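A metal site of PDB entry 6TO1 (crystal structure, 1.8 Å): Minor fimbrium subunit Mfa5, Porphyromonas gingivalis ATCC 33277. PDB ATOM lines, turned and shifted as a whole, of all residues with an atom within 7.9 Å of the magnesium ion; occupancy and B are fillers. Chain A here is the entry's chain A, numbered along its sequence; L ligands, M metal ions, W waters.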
ATOM      1  N   ASP A 133      10.353  25.397 -21.964  1.00  0.00           N
ATOM      2  CA  ASP A 133      11.177  25.027 -20.812  1.00  0.00           C
ATOM      3  C   ASP A 133      11.230  23.502 -20.682  1.00  0.00           C
ATOM      4  O   ASP A 133      10.198  22.883 -20.453  1.00  0.00           O
ATOM      5  CB  ASP A 133      10.483  25.683 -19.620  1.00  0.00           C
ATOM      6  CG  ASP A 133      11.176  25.496 -18.299  1.00  0.00           C
ATOM      7  OD1 ASP A 133      12.106  24.673 -18.136  1.00  0.00           O
ATOM      8  OD2 ASP A 133      10.746  26.219 -17.379  1.00  0.00           O
ATOM      9  N   GLN A 134      12.409  22.906 -20.910  1.00  0.00           N
ATOM     10  CA  GLN A 134      12.625  21.483 -20.612  1.00  0.00           C
ATOM     11  C   GLN A 134      13.618  21.301 -19.467  1.00  0.00           C
ATOM     12  O   GLN A 134      14.417  20.352 -19.457  1.00  0.00           O
ATOM     13  CB  GLN A 134      13.081  20.712 -21.870  1.00  0.00           C
ATOM     14  CG  GLN A 134      14.401  21.094 -22.469  1.00  0.00           C
ATOM     15  CD  GLN A 134      14.915  20.067 -23.509  1.00  0.00           C
ATOM     16  OE1 GLN A 134      14.137  19.354 -24.143  1.00  0.00           O
ATOM     17  NE2 GLN A 134      16.216  20.004 -23.681  1.00  0.00           N
ATOM     18  N   SER A 135      13.604  22.216 -18.503  1.00  0.00           N
ATOM     19  CA  SER A 135      14.518  22.155 -17.361  1.00  0.00           C
ATOM     20  C   SER A 135      14.087  21.040 -16.417  1.00  0.00           C
ATOM     21  O   SER A 135      12.976  20.525 -16.483  1.00  0.00           O
ATOM     22  CB  SER A 135      14.549  23.488 -16.618  1.00  0.00           C
ATOM     23  OG  SER A 135      13.300  23.738 -16.003  1.00  0.00           O
ATOM     24  N   SER A 136      14.982  20.687 -15.489  1.00  0.00           N
ATOM     25  CA  SER A 136      14.722  19.544 -14.603  1.00  0.00           C
ATOM     26  C   SER A 136      13.520  19.769 -13.689  1.00  0.00           C
ATOM     27  O   SER A 136      12.836  18.803 -13.315  1.00  0.00           O
ATOM     28  CB  SER A 136      16.010  19.221 -13.810  1.00  0.00           C
ATOM     29  OG  SER A 136      16.110  19.985 -12.635  1.00  0.00           O
ATOM     30  N   SER A 137      13.186  21.036 -13.371  1.00  0.00           N
ATOM     31  CA  SER A 137      11.996  21.279 -12.567  1.00  0.00           C
ATOM     32  C   SER A 137      10.720  20.889 -13.283  1.00  0.00           C
ATOM     33  O   SER A 137       9.669  20.771 -12.621  1.00  0.00           O
ATOM     34  CB  SER A 137      11.941  22.764 -12.172  1.00  0.00           C
ATOM     35  OG  SER A 137      11.807  23.558 -13.356  1.00  0.00           O
ATOM     36  N   MET A 138      10.764  20.719 -14.613  1.00  0.00           N
ATOM     37  CA  MET A 138       9.633  20.235 -15.399  1.00  0.00           C
ATOM     38  C   MET A 138       9.587  18.701 -15.451  1.00  0.00           C
ATOM     39  O   MET A 138       8.629  18.151 -16.022  1.00  0.00           O
ATOM     40  CB  MET A 138       9.697  20.765 -16.851  1.00  0.00           C
ATOM     41  CG  MET A 138       9.718  22.302 -17.003  1.00  0.00           C
ATOM     42  SD  MET A 138       8.104  23.085 -16.854  1.00  0.00           S
ATOM     43  CE  MET A 138       7.278  22.570 -18.358  1.00  0.00           C
ATOM     44  N   GLY A 139      10.553  18.029 -14.836  1.00  0.00           N
ATOM     45  CA  GLY A 139      10.633  16.582 -14.826  1.00  0.00           C
ATOM     46  C   GLY A 139      10.682  15.962 -13.437  1.00  0.00           C
ATOM     47  O   GLY A 139      10.356  16.617 -12.452  1.00  0.00           O
ATOM     48  N   ASN A 142       7.911  16.273 -10.883  1.00  0.00           N
ATOM     49  CA  ASN A 142       7.048  17.217 -11.555  1.00  0.00           C
ATOM     50  C   ASN A 142       6.829  16.878 -13.021  1.00  0.00           C
ATOM     51  O   ASN A 142       6.432  17.756 -13.786  1.00  0.00           O
ATOM     52  CB  ASN A 142       7.611  18.639 -11.466  1.00  0.00           C
ATOM     53  CG  ASN A 142       7.846  19.102 -10.053  1.00  0.00           C
ATOM     54  OD1 ASN A 142       7.115  18.735  -9.141  1.00  0.00           O
ATOM     55  ND2 ASN A 142       8.867  19.936  -9.857  1.00  0.00           N
ATOM     56  N   ARG A 145       4.426  18.260 -15.570  1.00  0.00           N
ATOM     57  CA  ARG A 145       4.619  19.558 -16.207  1.00  0.00           C
ATOM     58  C   ARG A 145       5.108  19.395 -17.644  1.00  0.00           C
ATOM     59  O   ARG A 145       4.472  19.888 -18.586  1.00  0.00           O
ATOM     60  CB  ARG A 145       5.630  20.385 -15.398  1.00  0.00           C
ATOM     61  CG  ARG A 145       5.124  20.795 -14.022  1.00  0.00           C
ATOM     62  CD  ARG A 145       6.141  21.665 -13.284  1.00  0.00           C
ATOM     63  NE  ARG A 145       5.789  21.879 -11.883  1.00  0.00           N
ATOM     64  CZ  ARG A 145       6.564  22.512 -11.004  1.00  0.00           C
ATOM     65  NH1 ARG A 145       7.738  23.008 -11.382  1.00  0.00           N
ATOM     66  NH2 ARG A 145       6.180  22.655  -9.755  1.00  0.00           N
ATOM     67  N   TYR A 177      14.677  24.972 -24.124  1.00  0.00           N
ATOM     68  CA  TYR A 177      15.813  25.389 -23.355  1.00  0.00           C
ATOM     69  C   TYR A 177      15.881  24.664 -22.031  1.00  0.00           C
ATOM     70  O   TYR A 177      14.866  24.249 -21.444  1.00  0.00           O
ATOM     71  CB  TYR A 177      15.838  26.907 -23.113  1.00  0.00           C
ATOM     72  CG  TYR A 177      14.748  27.421 -22.195  1.00  0.00           C
ATOM     73  CD1 TYR A 177      14.963  27.589 -20.834  1.00  0.00           C
ATOM     74  CD2 TYR A 177      13.505  27.763 -22.691  1.00  0.00           C
ATOM     75  CE1 TYR A 177      13.978  28.060 -20.013  1.00  0.00           C
ATOM     76  CE2 TYR A 177      12.514  28.225 -21.861  1.00  0.00           C
ATOM     77  CZ  TYR A 177      12.760  28.381 -20.526  1.00  0.00           C
ATOM     78  OH  TYR A 177      11.759  28.869 -19.697  1.00  0.00           O
ATOM     79  N   ASP A 178      17.112  24.512 -21.573  1.00  0.00           N
ATOM     80  CA  ASP A 178      17.433  24.081 -20.218  1.00  0.00           C
ATOM     81  C   ASP A 178      18.503  25.052 -19.709  1.00  0.00           C
ATOM     82  O   ASP A 178      18.222  26.244 -19.533  1.00  0.00           O
ATOM     83  CB  ASP A 178      17.900  22.620 -20.191  1.00  0.00           C
ATOM     84  CG  ASP A 178      18.857  22.265 -21.322  1.00  0.00           C
ATOM     85  OD1 ASP A 178      20.049  22.624 -21.219  1.00  0.00           O
ATOM     86  OD2 ASP A 178      18.384  21.613 -22.314  1.00  0.00           O
ATOM     87  N   ILE A 204      16.384  18.488 -18.517  1.00  0.00           N
ATOM     88  CA  ILE A 204      17.807  18.716 -18.351  1.00  0.00           C
ATOM     89  C   ILE A 204      17.991  19.827 -17.340  1.00  0.00           C
ATOM     90  O   ILE A 204      17.203  20.782 -17.318  1.00  0.00           O
ATOM     91  CB  ILE A 204      18.487  19.079 -19.692  1.00  0.00           C
ATOM     92  CG1 ILE A 204      18.361  17.910 -20.675  1.00  0.00           C
ATOM     93  CG2 ILE A 204      19.924  19.453 -19.490  1.00  0.00           C
ATOM     94  CD1 ILE A 204      18.889  18.209 -22.072  1.00  0.00           C
ATOM     95  N   TRP A 205      19.006  19.729 -16.487  1.00  0.00           N
ATOM     96  CA  TRP A 205      19.187  20.721 -15.431  1.00  0.00           C
ATOM     97  C   TRP A 205      19.305  22.137 -16.021  1.00  0.00           C
ATOM     98  O   TRP A 205      19.902  22.347 -17.085  1.00  0.00           O
ATOM     99  CB  TRP A 205      20.444  20.421 -14.572  1.00  0.00           C
ATOM    100  CG  TRP A 205      21.773  20.422 -15.307  1.00  0.00           C
ATOM    101  CD1 TRP A 205      22.409  19.357 -15.918  1.00  0.00           C
ATOM    102  CD2 TRP A 205      22.635  21.569 -15.535  1.00  0.00           C
ATOM    103  NE1 TRP A 205      23.569  19.775 -16.517  1.00  0.00           N
ATOM    104  CE2 TRP A 205      23.746  21.109 -16.281  1.00  0.00           C
ATOM    105  CE3 TRP A 205      22.575  22.904 -15.166  1.00  0.00           C
ATOM    106  CZ2 TRP A 205      24.760  21.966 -16.681  1.00  0.00           C
ATOM    107  CZ3 TRP A 205      23.588  23.752 -15.586  1.00  0.00           C
ATOM    108  CH2 TRP A 205      24.670  23.281 -16.315  1.00  0.00           C
ATOM    109  N   GLY A 206      18.797  23.113 -15.271  1.00  0.00           N
ATOM    110  CA  GLY A 206      19.034  24.507 -15.603  1.00  0.00           C
ATOM    111  C   GLY A 206      17.840  25.135 -16.285  1.00  0.00           C
ATOM    112  O   GLY A 206      17.237  24.504 -17.142  1.00  0.00           O
ATOM    113  N   THR A 207      17.492  26.376 -15.948  1.00  0.00           N
ATOM    114  CA  THR A 207      16.337  27.052 -16.535  1.00  0.00           C
ATOM    115  C   THR A 207      16.785  28.424 -17.033  1.00  0.00           C
ATOM    116  O   THR A 207      16.624  29.448 -16.343  1.00  0.00           O
ATOM    117  CB  THR A 207      15.183  27.135 -15.530  1.00  0.00           C
ATOM    118  OG1 THR A 207      14.883  25.851 -14.957  1.00  0.00           O
ATOM    119  CG2 THR A 207      13.942  27.708 -16.205  1.00  0.00           C
ATOM    120  N   HIS A 208      17.320  28.466 -18.250  1.00  0.00           N
ATOM    121  CA  HIS A 208      17.905  29.694 -18.836  1.00  0.00           C
ATOM    122  C   HIS A 208      16.839  30.391 -19.686  1.00  0.00           C
ATOM    123  O   HIS A 208      16.895  30.409 -20.920  1.00  0.00           O
ATOM    124  CB  HIS A 208      19.130  29.327 -19.642  1.00  0.00           C
ATOM    125  CG  HIS A 208      20.122  30.430 -19.842  1.00  0.00           C
ATOM    126  ND1 HIS A 208      19.778  31.713 -20.201  1.00  0.00           N
ATOM    127  CD2 HIS A 208      21.477  30.417 -19.767  1.00  0.00           C
ATOM    128  CE1 HIS A 208      20.867  32.447 -20.336  1.00  0.00           C
ATOM    129  NE2 HIS A 208      21.916  31.681 -20.061  1.00  0.00           N
ATOM    130  N   THR A 209      15.814  30.903 -19.003  1.00  0.00           N
ATOM    131  CA  THR A 209      14.679  31.485 -19.706  1.00  0.00           C
ATOM    132  C   THR A 209      15.118  32.671 -20.561  1.00  0.00           C
ATOM    133  O   THR A 209      14.666  32.839 -21.700  1.00  0.00           O
ATOM    134  CB  THR A 209      13.600  31.851 -18.691  1.00  0.00           C
ATOM    135  OG1 THR A 209      13.265  30.667 -17.944  1.00  0.00           O
ATOM    136  CG2 THR A 209      12.339  32.411 -19.338  1.00  0.00           C
ATOM    137  N   SER A 234       6.545  27.632 -19.593  1.00  0.00           N
ATOM    138  CA  SER A 234       7.548  27.438 -18.557  1.00  0.00           C
ATOM    139  C   SER A 234       6.858  27.252 -17.223  1.00  0.00           C
ATOM    140  O   SER A 234       5.732  27.707 -17.024  1.00  0.00           O
ATOM    141  CB  SER A 234       8.515  28.634 -18.522  1.00  0.00           C
ATOM    142  OG  SER A 234       9.381  28.529 -17.404  1.00  0.00           O
ATOM    143  N   ASP A 235       7.551  26.615 -16.270  1.00  0.00           N
ATOM    144  CA  ASP A 235       6.957  26.650 -14.942  1.00  0.00           C
ATOM    145  C   ASP A 235       7.279  27.947 -14.203  1.00  0.00           C
ATOM    146  O   ASP A 235       6.739  28.159 -13.117  1.00  0.00           O
ATOM    147  CB  ASP A 235       7.341  25.440 -14.087  1.00  0.00           C
ATOM    148  CG  ASP A 235       8.814  25.340 -13.783  1.00  0.00           C
ATOM    149  OD1 ASP A 235       9.519  26.386 -13.663  1.00  0.00           O
ATOM    150  OD2 ASP A 235       9.274  24.174 -13.666  1.00  0.00           O
ATOM    151  N   GLY A 236       8.115  28.818 -14.777  1.00  0.00           N
ATOM    152  CA  GLY A 236       8.223  30.188 -14.328  1.00  0.00           C
ATOM    153  C   GLY A 236       9.386  30.504 -13.421  1.00  0.00           C
ATOM    154  O   GLY A 236       9.623  31.692 -13.122  1.00  0.00           O
ATOM    155  N   LEU A 237      10.097  29.508 -12.926  1.00  0.00           N
ATOM    156  CA  LEU A 237      11.236  29.758 -12.051  1.00  0.00           C
ATOM    157  C   LEU A 237      12.541  29.715 -12.828  1.00  0.00           C
ATOM    158  O   LEU A 237      13.169  28.657 -12.956  1.00  0.00           O
ATOM    159  CB  LEU A 237      11.233  28.762 -10.897  1.00  0.00           C
ATOM    160  CG  LEU A 237      12.304  29.016  -9.838  1.00  0.00           C
ATOM    161  CD1 LEU A 237      12.081  30.428  -9.240  1.00  0.00           C
ATOM    162  CD2 LEU A 237      12.365  27.972  -8.746  1.00  0.00           C
ATOM    163  N   ALA A 238      12.984  30.872 -13.328  1.00  0.00           N
ATOM    164  CA  ALA A 238      14.261  30.916 -14.031  1.00  0.00           C
ATOM    165  C   ALA A 238      15.413  30.746 -13.048  1.00  0.00           C
ATOM    166  O   ALA A 238      15.374  31.244 -11.921  1.00  0.00           O
ATOM    167  CB  ALA A 238      14.408  32.236 -14.816  1.00  0.00           C
ATOM    168  N   THR A 239      16.431  30.015 -13.473  1.00  0.00           N
ATOM    169  CA  THR A 239      17.558  29.749 -12.611  1.00  0.00           C
ATOM    170  C   THR A 239      18.917  29.996 -13.270  1.00  0.00           C
ATOM    171  O   THR A 239      19.948  29.742 -12.632  1.00  0.00           O
ATOM    172  CB  THR A 239      17.521  28.289 -12.100  1.00  0.00           C
ATOM    173  OG1 THR A 239      17.584  27.389 -13.210  1.00  0.00           O
ATOM    174  CG2 THR A 239      16.284  28.019 -11.274  1.00  0.00           C
HETATM  175  P1  LIG L   1      16.052  23.590 -12.870  1.00  0.00           P
HETATM  176  O1  LIG L   1      16.888  22.405 -13.392  1.00  0.00           O
HETATM  177  O2  LIG L   1      16.767  24.899 -13.192  1.00  0.00           O
HETATM  178  O3  LIG L   1      15.971  23.447 -11.363  1.00  0.00           O
HETATM  179  O4  LIG L   1      14.670  23.546 -13.400  1.00  0.00           O
HETATM  180 MG    MG M   1      13.313  24.757 -14.192  1.00  0.00          MG
HETATM  181  O   HOH W   1      13.166  25.964 -12.468  1.00  0.00           O
HETATM  182  O   HOH W   2      11.774  25.881 -14.893  1.00  0.00           O
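The backbone carbonyl oxygen (O) of Ser 137 lies within hydrogen-bond range of the guanidinium group (NH1) of Arg 145 (3.2 Å). The backbone NH (N) of Ser 135 lies within hydrogen-bond range of the side-chain carboxylate (OD1) of Asp 133. OD2 of Asp 235 sits close to OG of Ser 137 (2.6 Å). The side-chain hydroxyl of Thr 239 is in hydrogen-bond range of the backbone NH of Thr 207, 2.9 Å away. ND2 of Asn 142 sits at hydrogen-bond distance from O of Ser 137 (3.0 Å).
Within 4 Å of the magnesium ion: Ser 135, Ser 137 and Thr 207.
The magnesium ion is bound by an oxygen (O4) of the ligand (2.0 Å), water W2 (2.0 Å), the side-chain hydroxyl of Thr 207 (2.1 Å), the side-chain hydroxyl of Ser 135 (2.1 Å), the side-chain hydroxyl of Ser 137 (2.1 Å) and water W1 (2.1 Å). The magnesium ion has six donor atoms within binding distance.
Water W2 lies within hydrogen-bond range of OD1 of Asp 235 (2.6 Å) and OD2 of Asp 133 (2.7 Å).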
